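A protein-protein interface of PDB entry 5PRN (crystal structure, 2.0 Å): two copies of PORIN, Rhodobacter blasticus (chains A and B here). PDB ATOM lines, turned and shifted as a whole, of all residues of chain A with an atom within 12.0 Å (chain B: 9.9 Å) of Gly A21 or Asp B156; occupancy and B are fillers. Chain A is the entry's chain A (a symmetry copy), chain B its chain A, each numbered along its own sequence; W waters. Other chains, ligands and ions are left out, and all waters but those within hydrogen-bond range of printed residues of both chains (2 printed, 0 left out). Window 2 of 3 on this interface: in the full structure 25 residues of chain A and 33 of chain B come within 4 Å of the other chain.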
ATOM      1  N   TYR A  14     -24.317  29.994 -20.685  1.00  0.00           N
ATOM      2  CA  TYR A  14     -25.053  29.125 -19.761  1.00  0.00           C
ATOM      3  C   TYR A  14     -26.522  29.027 -20.169  1.00  0.00           C
ATOM      4  O   TYR A  14     -27.204  30.033 -20.414  1.00  0.00           O
ATOM      5  CB  TYR A  14     -24.950  29.662 -18.330  1.00  0.00           C
ATOM      6  CG  TYR A  14     -25.871  29.013 -17.304  1.00  0.00           C
ATOM      7  CD1 TYR A  14     -25.592  27.769 -16.745  1.00  0.00           C
ATOM      8  CD2 TYR A  14     -27.048  29.646 -16.935  1.00  0.00           C
ATOM      9  CE1 TYR A  14     -26.441  27.171 -15.793  1.00  0.00           C
ATOM     10  CE2 TYR A  14     -27.916  29.080 -15.999  1.00  0.00           C
ATOM     11  CZ  TYR A  14     -27.587  27.854 -15.426  1.00  0.00           C
ATOM     12  OH  TYR A  14     -28.474  27.322 -14.505  1.00  0.00           O
ATOM     13  N   VAL A  15     -26.996  27.778 -20.249  1.00  0.00           N
ATOM     14  CA  VAL A  15     -28.369  27.438 -20.575  1.00  0.00           C
ATOM     15  C   VAL A  15     -28.872  26.501 -19.442  1.00  0.00           C
ATOM     16  O   VAL A  15     -28.301  25.409 -19.281  1.00  0.00           O
ATOM     17  CB  VAL A  15     -28.579  26.780 -21.923  1.00  0.00           C
ATOM     18  CG1 VAL A  15     -30.086  26.483 -22.119  1.00  0.00           C
ATOM     19  CG2 VAL A  15     -28.105  27.683 -23.078  1.00  0.00           C
ATOM     20  N   GLU A  16     -29.744  27.002 -18.575  1.00  0.00           N
ATOM     21  CA  GLU A  16     -30.184  26.174 -17.429  1.00  0.00           C
ATOM     22  C   GLU A  16     -30.820  24.871 -17.914  1.00  0.00           C
ATOM     23  O   GLU A  16     -31.727  24.908 -18.750  1.00  0.00           O
ATOM     24  CB  GLU A  16     -31.199  26.942 -16.577  1.00  0.00           C
ATOM     25  CG  GLU A  16     -31.504  26.204 -15.265  1.00  0.00           C
ATOM     26  CD  GLU A  16     -32.438  26.917 -14.321  1.00  0.00           C
ATOM     27  OE1 GLU A  16     -33.010  27.988 -14.586  1.00  0.00           O
ATOM     28  OE2 GLU A  16     -32.601  26.351 -13.206  1.00  0.00           O
ATOM     29  N   ASP A  17     -30.318  23.740 -17.411  1.00  0.00           N
ATOM     30  CA  ASP A  17     -30.842  22.439 -17.813  1.00  0.00           C
ATOM     31  C   ASP A  17     -30.877  22.289 -19.314  1.00  0.00           C
ATOM     32  O   ASP A  17     -31.927  21.974 -19.888  1.00  0.00           O
ATOM     33  CB  ASP A  17     -32.265  22.182 -17.291  1.00  0.00           C
ATOM     34  CG  ASP A  17     -32.377  22.174 -15.793  1.00  0.00           C
ATOM     35  OD1 ASP A  17     -31.415  21.811 -15.066  1.00  0.00           O
ATOM     36  OD2 ASP A  17     -33.477  22.579 -15.303  1.00  0.00           O
ATOM     37  N   ARG A  18     -29.736  22.435 -19.977  1.00  0.00           N
ATOM     38  CA  ARG A  18     -29.649  22.306 -21.429  1.00  0.00           C
ATOM     39  C   ARG A  18     -30.071  20.971 -21.994  1.00  0.00           C
ATOM     40  O   ARG A  18     -30.607  20.887 -23.128  1.00  0.00           O
ATOM     41  CB  ARG A  18     -28.183  22.631 -21.774  1.00  0.00           C
ATOM     42  CG  ARG A  18     -27.883  23.032 -23.210  1.00  0.00           C
ATOM     43  CD  ARG A  18     -26.364  23.059 -23.481  1.00  0.00           C
ATOM     44  NE  ARG A  18     -25.671  24.217 -22.883  1.00  0.00           N
ATOM     45  CZ  ARG A  18     -25.464  25.374 -23.529  1.00  0.00           C
ATOM     46  NH1 ARG A  18     -25.899  25.547 -24.785  1.00  0.00           N
ATOM     47  NH2 ARG A  18     -24.824  26.423 -22.997  1.00  0.00           N
ATOM     48  N   GLY A  19     -29.856  19.849 -21.304  1.00  0.00           N
ATOM     49  CA  GLY A  19     -30.251  18.558 -21.943  1.00  0.00           C
ATOM     50  C   GLY A  19     -29.628  17.423 -21.152  1.00  0.00           C
ATOM     51  O   GLY A  19     -28.622  17.615 -20.453  1.00  0.00           O
ATOM     52  N   VAL A  20     -30.247  16.247 -21.259  1.00  0.00           N
ATOM     53  CA  VAL A  20     -29.764  15.059 -20.539  1.00  0.00           C
ATOM     54  C   VAL A  20     -28.325  14.743 -20.922  1.00  0.00           C
ATOM     55  O   VAL A  20     -28.070  14.564 -22.104  1.00  0.00           O
ATOM     56  CB  VAL A  20     -30.677  13.860 -20.890  1.00  0.00           C
ATOM     57  CG1 VAL A  20     -30.049  12.514 -20.552  1.00  0.00           C
ATOM     58  CG2 VAL A  20     -31.992  13.999 -20.109  1.00  0.00           C
ATOM     59  N   GLY A  21     -27.427  14.675 -19.945  1.00  0.00           N
ATOM     60  CA  GLY A  21     -26.031  14.376 -20.230  1.00  0.00           C
ATOM     61  C   GLY A  21     -25.275  15.484 -20.958  1.00  0.00           C
ATOM     62  O   GLY A  21     -24.255  15.170 -21.593  1.00  0.00           O
ATOM     63  N   LEU A  22     -25.741  16.729 -20.891  1.00  0.00           N
ATOM     64  CA  LEU A  22     -25.083  17.856 -21.526  1.00  0.00           C
ATOM     65  C   LEU A  22     -24.627  18.822 -20.433  1.00  0.00           C
ATOM     66  O   LEU A  22     -25.259  18.992 -19.403  1.00  0.00           O
ATOM     67  CB  LEU A  22     -25.922  18.631 -22.532  1.00  0.00           C
ATOM     68  CG  LEU A  22     -26.433  17.905 -23.767  1.00  0.00           C
ATOM     69  CD1 LEU A  22     -27.396  18.804 -24.550  1.00  0.00           C
ATOM     70  CD2 LEU A  22     -25.320  17.430 -24.683  1.00  0.00           C
ATOM     71  N   GLU A  23     -23.516  19.485 -20.688  1.00  0.00           N
ATOM     72  CA  GLU A  23     -23.020  20.513 -19.764  1.00  0.00           C
ATOM     73  C   GLU A  23     -23.898  21.752 -19.945  1.00  0.00           C
ATOM     74  O   GLU A  23     -24.187  22.147 -21.072  1.00  0.00           O
ATOM     75  CB  GLU A  23     -21.594  20.858 -20.135  1.00  0.00           C
ATOM     76  CG  GLU A  23     -20.404  20.355 -19.316  1.00  0.00           C
ATOM     77  CD  GLU A  23     -20.642  20.040 -17.858  1.00  0.00           C
ATOM     78  OE1 GLU A  23     -21.358  20.794 -17.114  1.00  0.00           O
ATOM     79  OE2 GLU A  23     -20.092  18.971 -17.394  1.00  0.00           O
ATOM     80  N   ASP A  24     -24.333  22.402 -18.889  1.00  0.00           N
ATOM     81  CA  ASP A  24     -25.159  23.594 -19.013  1.00  0.00           C
ATOM     82  C   ASP A  24     -24.285  24.801 -19.442  1.00  0.00           C
ATOM     83  O   ASP A  24     -24.797  25.669 -20.163  1.00  0.00           O
ATOM     84  CB  ASP A  24     -25.708  23.970 -17.631  1.00  0.00           C
ATOM     85  CG  ASP A  24     -26.982  23.149 -17.299  1.00  0.00           C
ATOM     86  OD1 ASP A  24     -27.561  22.493 -18.182  1.00  0.00           O
ATOM     87  OD2 ASP A  24     -27.381  23.306 -16.143  1.00  0.00           O
ATOM     88  N   THR A  25     -23.061  24.810 -18.958  1.00  0.00           N
ATOM     89  CA  THR A  25     -22.137  25.895 -19.283  1.00  0.00           C
ATOM     90  C   THR A  25     -21.057  25.467 -20.259  1.00  0.00           C
ATOM     91  O   THR A  25     -20.375  24.438 -20.048  1.00  0.00           O
ATOM     92  CB  THR A  25     -21.492  26.480 -18.007  1.00  0.00           C
ATOM     93  OG1 THR A  25     -22.546  27.027 -17.193  1.00  0.00           O
ATOM     94  CG2 THR A  25     -20.563  27.674 -18.349  1.00  0.00           C
ATOM     95  N   ILE A  26     -20.922  26.162 -21.397  1.00  0.00           N
ATOM     96  CA  ILE A  26     -19.860  25.878 -22.348  1.00  0.00           C
ATOM     97  C   ILE A  26     -19.112  27.204 -22.713  1.00  0.00           C
ATOM     98  O   ILE A  26     -19.533  28.302 -22.343  1.00  0.00           O
ATOM     99  CB  ILE A  26     -20.347  25.279 -23.703  1.00  0.00           C
ATOM    100  CG1 ILE A  26     -21.190  26.299 -24.443  1.00  0.00           C
ATOM    101  CG2 ILE A  26     -21.071  23.959 -23.478  1.00  0.00           C
ATOM    102  CD1 ILE A  26     -21.772  25.929 -25.764  1.00  0.00           C
ATOM    103  N   ILE A  27     -17.957  27.046 -23.343  1.00  0.00           N
ATOM    104  CA  ILE A  27     -17.195  28.217 -23.814  1.00  0.00           C
ATOM    105  C   ILE A  27     -17.603  28.436 -25.264  1.00  0.00           C
ATOM    106  O   ILE A  27     -17.308  27.596 -26.146  1.00  0.00           O
ATOM    107  CB  ILE A  27     -15.679  28.045 -23.692  1.00  0.00           C
ATOM    108  CG1 ILE A  27     -15.353  28.019 -22.177  1.00  0.00           C
ATOM    109  CG2 ILE A  27     -14.869  29.125 -24.400  1.00  0.00           C
ATOM    110  CD1 ILE A  27     -13.981  27.327 -21.968  1.00  0.00           C
ATOM    111  N   TYR B 148      -5.035  22.474 -21.033  1.00  0.00           N
ATOM    112  CA  TYR B 148      -6.174  21.654 -20.695  1.00  0.00           C
ATOM    113  C   TYR B 148      -7.023  21.479 -21.945  1.00  0.00           C
ATOM    114  O   TYR B 148      -7.394  22.502 -22.559  1.00  0.00           O
ATOM    115  CB  TYR B 148      -6.963  22.394 -19.605  1.00  0.00           C
ATOM    116  CG  TYR B 148      -8.342  21.825 -19.415  1.00  0.00           C
ATOM    117  CD1 TYR B 148      -8.555  20.639 -18.747  1.00  0.00           C
ATOM    118  CD2 TYR B 148      -9.439  22.489 -19.927  1.00  0.00           C
ATOM    119  CE1 TYR B 148      -9.821  20.108 -18.568  1.00  0.00           C
ATOM    120  CE2 TYR B 148     -10.725  22.000 -19.757  1.00  0.00           C
ATOM    121  CZ  TYR B 148     -10.902  20.806 -19.080  1.00  0.00           C
ATOM    122  OH  TYR B 148     -12.193  20.343 -18.923  1.00  0.00           O
ATOM    123  N   ASP B 150     -10.356  19.636 -23.664  1.00  0.00           N
ATOM    124  CA  ASP B 150     -11.572  18.802 -23.502  1.00  0.00           C
ATOM    125  C   ASP B 150     -12.012  18.397 -24.914  1.00  0.00           C
ATOM    126  O   ASP B 150     -12.386  19.259 -25.703  1.00  0.00           O
ATOM    127  CB  ASP B 150     -12.604  19.700 -22.842  1.00  0.00           C
ATOM    128  CG  ASP B 150     -13.903  18.982 -22.476  1.00  0.00           C
ATOM    129  OD1 ASP B 150     -14.131  17.883 -22.974  1.00  0.00           O
ATOM    130  OD2 ASP B 150     -14.693  19.601 -21.732  1.00  0.00           O
ATOM    131  N   PRO B 151     -11.979  17.117 -25.261  1.00  0.00           N
ATOM    132  CA  PRO B 151     -12.348  16.622 -26.556  1.00  0.00           C
ATOM    133  C   PRO B 151     -13.767  16.885 -26.964  1.00  0.00           C
ATOM    134  O   PRO B 151     -14.114  16.884 -28.168  1.00  0.00           O
ATOM    135  CB  PRO B 151     -12.123  15.093 -26.500  1.00  0.00           C
ATOM    136  CG  PRO B 151     -11.506  14.804 -25.187  1.00  0.00           C
ATOM    137  CD  PRO B 151     -11.531  16.034 -24.331  1.00  0.00           C
ATOM    138  N   ASP B 152     -14.712  17.036 -26.049  1.00  0.00           N
ATOM    139  CA  ASP B 152     -16.082  17.334 -26.378  1.00  0.00           C
ATOM    140  C   ASP B 152     -16.643  18.129 -25.201  1.00  0.00           C
ATOM    141  O   ASP B 152     -17.178  17.522 -24.245  1.00  0.00           O
ATOM    142  CB  ASP B 152     -16.992  16.106 -26.634  1.00  0.00           C
ATOM    143  CG  ASP B 152     -18.359  16.550 -27.096  1.00  0.00           C
ATOM    144  OD1 ASP B 152     -18.880  17.662 -26.775  1.00  0.00           O
ATOM    145  OD2 ASP B 152     -19.019  15.791 -27.831  1.00  0.00           O
ATOM    146  N   GLN B 153     -16.545  19.472 -25.318  1.00  0.00           N
ATOM    147  CA  GLN B 153     -17.018  20.277 -24.180  1.00  0.00           C
ATOM    148  C   GLN B 153     -18.505  20.314 -23.978  1.00  0.00           C
ATOM    149  O   GLN B 153     -18.960  20.886 -22.974  1.00  0.00           O
ATOM    150  CB  GLN B 153     -16.442  21.731 -24.348  1.00  0.00           C
ATOM    151  CG  GLN B 153     -17.219  22.525 -25.441  1.00  0.00           C
ATOM    152  CD  GLN B 153     -17.029  24.024 -25.299  1.00  0.00           C
ATOM    153  OE1 GLN B 153     -16.741  24.562 -24.194  1.00  0.00           O
ATOM    154  NE2 GLN B 153     -17.196  24.761 -26.397  1.00  0.00           N
ATOM    155  N   THR B 154     -19.368  19.825 -24.839  1.00  0.00           N
ATOM    156  CA  THR B 154     -20.786  19.900 -24.697  1.00  0.00           C
ATOM    157  C   THR B 154     -21.312  18.754 -23.797  1.00  0.00           C
ATOM    158  O   THR B 154     -22.356  18.915 -23.169  1.00  0.00           O
ATOM    159  CB  THR B 154     -21.549  19.854 -26.041  1.00  0.00           C
ATOM    160  OG1 THR B 154     -21.312  18.578 -26.624  1.00  0.00           O
ATOM    161  CG2 THR B 154     -21.060  20.929 -27.031  1.00  0.00           C
ATOM    162  N   VAL B 155     -20.595  17.663 -23.718  1.00  0.00           N
ATOM    163  CA  VAL B 155     -21.089  16.466 -22.977  1.00  0.00           C
ATOM    164  C   VAL B 155     -20.668  16.515 -21.538  1.00  0.00           C
ATOM    165  O   VAL B 155     -19.605  17.047 -21.188  1.00  0.00           O
ATOM    166  CB  VAL B 155     -20.477  15.227 -23.696  1.00  0.00           C
ATOM    167  CG1 VAL B 155     -20.586  13.977 -22.856  1.00  0.00           C
ATOM    168  CG2 VAL B 155     -21.190  15.032 -25.039  1.00  0.00           C
ATOM    169  N   ASP B 156     -21.497  15.982 -20.609  1.00  0.00           N
ATOM    170  CA  ASP B 156     -21.135  15.996 -19.196  1.00  0.00           C
ATOM    171  C   ASP B 156     -19.681  15.572 -19.004  1.00  0.00           C
ATOM    172  O   ASP B 156     -19.320  14.506 -19.518  1.00  0.00           O
ATOM    173  CB  ASP B 156     -22.016  14.949 -18.436  1.00  0.00           C
ATOM    174  CG  ASP B 156     -21.908  15.219 -16.940  1.00  0.00           C
ATOM    175  OD1 ASP B 156     -20.840  14.873 -16.303  1.00  0.00           O
ATOM    176  OD2 ASP B 156     -22.861  15.826 -16.328  1.00  0.00           O
ATOM    177  N   SER B 157     -18.887  16.275 -18.229  1.00  0.00           N
ATOM    178  CA  SER B 157     -17.480  16.004 -18.057  1.00  0.00           C
ATOM    179  C   SER B 157     -17.046  14.698 -17.450  1.00  0.00           C
ATOM    180  O   SER B 157     -15.902  14.275 -17.703  1.00  0.00           O
ATOM    181  CB  SER B 157     -16.818  17.146 -17.231  1.00  0.00           C
ATOM    182  OG  SER B 157     -17.117  18.397 -17.834  1.00  0.00           O
ATOM    183  N   SER B 158     -17.909  13.980 -16.744  1.00  0.00           N
ATOM    184  CA  SER B 158     -17.533  12.693 -16.135  1.00  0.00           C
ATOM    185  C   SER B 158     -17.595  11.606 -17.180  1.00  0.00           C
ATOM    186  O   SER B 158     -17.101  10.476 -17.007  1.00  0.00           O
ATOM    187  CB  SER B 158     -18.483  12.414 -14.957  1.00  0.00           C
ATOM    188  OG  SER B 158     -19.791  12.204 -15.492  1.00  0.00           O
ATOM    189  N   LEU B 159     -18.176  11.925 -18.331  1.00  0.00           N
ATOM    190  CA  LEU B 159     -18.233  11.009 -19.444  1.00  0.00           C
ATOM    191  C   LEU B 159     -17.110  11.183 -20.456  1.00  0.00           C
ATOM    192  O   LEU B 159     -17.039  10.435 -21.450  1.00  0.00           O
ATOM    193  CB  LEU B 159     -19.596  11.269 -20.158  1.00  0.00           C
ATOM    194  CG  LEU B 159     -20.772  11.073 -19.155  1.00  0.00           C
ATOM    195  CD1 LEU B 159     -22.071  11.595 -19.702  1.00  0.00           C
ATOM    196  CD2 LEU B 159     -20.892   9.592 -18.807  1.00  0.00           C
ATOM    197  N   VAL B 160     -16.263  12.202 -20.313  1.00  0.00           N
ATOM    198  CA  VAL B 160     -15.195  12.442 -21.297  1.00  0.00           C
ATOM    199  C   VAL B 160     -13.841  12.456 -20.588  1.00  0.00           C
ATOM    200  O   VAL B 160     -13.765  12.840 -19.417  1.00  0.00           O
ATOM    201  CB  VAL B 160     -15.358  13.811 -22.004  1.00  0.00           C
ATOM    202  CG1 VAL B 160     -14.428  13.980 -23.199  1.00  0.00           C
ATOM    203  CG2 VAL B 160     -16.793  14.078 -22.435  1.00  0.00           C
ATOM    204  N   THR B 161     -12.797  12.056 -21.282  1.00  0.00           N
ATOM    205  CA  THR B 161     -11.460  12.092 -20.653  1.00  0.00           C
ATOM    206  C   THR B 161     -10.766  13.367 -21.111  1.00  0.00           C
ATOM    207  O   THR B 161     -10.578  13.457 -22.324  1.00  0.00           O
ATOM    208  CB  THR B 161     -10.633  10.877 -21.142  1.00  0.00           C
ATOM    209  OG1 THR B 161     -11.314   9.685 -20.750  1.00  0.00           O
ATOM    210  CG2 THR B 161      -9.236  10.892 -20.576  1.00  0.00           C
ATOM    211  N   GLU B 162     -10.413  14.269 -20.243  1.00  0.00           N
ATOM    212  CA  GLU B 162      -9.751  15.503 -20.610  1.00  0.00           C
ATOM    213  C   GLU B 162      -8.236  15.379 -20.428  1.00  0.00           C
ATOM    214  O   GLU B 162      -7.779  14.666 -19.545  1.00  0.00           O
ATOM    215  CB  GLU B 162     -10.229  16.685 -19.755  1.00  0.00           C
ATOM    216  CG  GLU B 162     -11.737  16.870 -19.856  1.00  0.00           C
ATOM    217  CD  GLU B 162     -12.422  16.437 -18.571  1.00  0.00           C
ATOM    218  OE1 GLU B 162     -11.776  16.087 -17.573  1.00  0.00           O
ATOM    219  OE2 GLU B 162     -13.666  16.485 -18.607  1.00  0.00           O
HETATM  220  O   HOH W   1     -18.399  22.504 -20.808  1.00  0.00           O
HETATM  221  O   HOH W   2     -23.540  21.333 -23.566  1.00  0.00           O
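OD1 of Asp B152 is in hydrogen-bond range of OG1 of Thr B154 (2.6 Å).
OG of Ser B158 lies within hydrogen-bond range of OD1 of Asp B156 (3.0 Å).
The guanidinium group of Arg A18 is in hydrogen-bond range of the backbone carbonyl oxygen of Glu A23 (3.1 Å).
Among the printed residues, merely in contact across the chains: Leu A22 with Thr B154 (3.4 Å), Glu A23 with Asp B156 (3.6 Å), Gly A21 with Val B155 (3.7 Å), Ile A26 with Gln B153 (3.7 Å), Glu A23 with Gln B153 (3.9 Å) and Glu A23 with Val B155 (3.9 Å).
No position is printed for both chains.
Of the 14 printed residues of chain B, 5 touch a printed residue of chain A.
Of the 14 printed residues of chain A, 5 touch a printed residue of chain B.
Hydrophobic or aromatic side chains of chain A that line the printed part of chain B: Leu A22, Ile A26 and Ile A27.
Along chain A the printed residues that touch a printed residue of chain B span positions 21 to 27.
No residue of chain B comes within 4 Å of Val A20.
Leu A22 touches just one residue of chain B: Thr B154 (3.4 Å).
Of the printed residues of chain B, Glu A23 touches Gln B153, Thr B154, Val B155, Asp B156 and Ser B157.
Printed residues of chain A within 4 Å of Gln B153: Glu A23, Ile A26 and Ile A27.
Of chain A, only Gly A21 and Glu A23 come within 4 Å of Val B155.
Asp B156 touches just these residues of chain A: Gly A21 and Glu A23.
Ser B157 touches one residue of chain A.
No residue of chain A comes within 4 Å of Ser B158.
No residue of chain A comes within 4 Å of Leu B159.
The nearest residue of chain B that does not touch Gly A21 is Thr B154 (4.5 Å).
The nearest printed residue of chain B that does not touch Glu A23 is Ser B158 (5.5 Å).
The side-chain amide nitrogen (NE2) of Gln B153 lies within hydrogen-bond range of the backbone carbonyl oxygen (O) of Ile A27 (2.8 Å).
N of Glu A23 sits at hydrogen-bond distance from O of Thr B154 (2.8 Å).
The backbone NH (N) of Asp B156 lies within hydrogen-bond range of the backbone carbonyl oxygen (O) of Gly A21, at 3.0 Å.
The side-chain carboxylate (OE2) of Glu A23 is in hydrogen-bond range of the side-chain hydroxyl (OG) of Ser B157.
Water W2 lies within hydrogen-bond range of the backbone carbonyl oxygen (O) of Glu A23 (2.7 Å) and the backbone carbonyl oxygen (O) of Thr B154 (2.7 Å).
Water W1 bridges the backbone carbonyl oxygen of Gln B153 and the backbone carbonyl oxygen of Thr A25.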
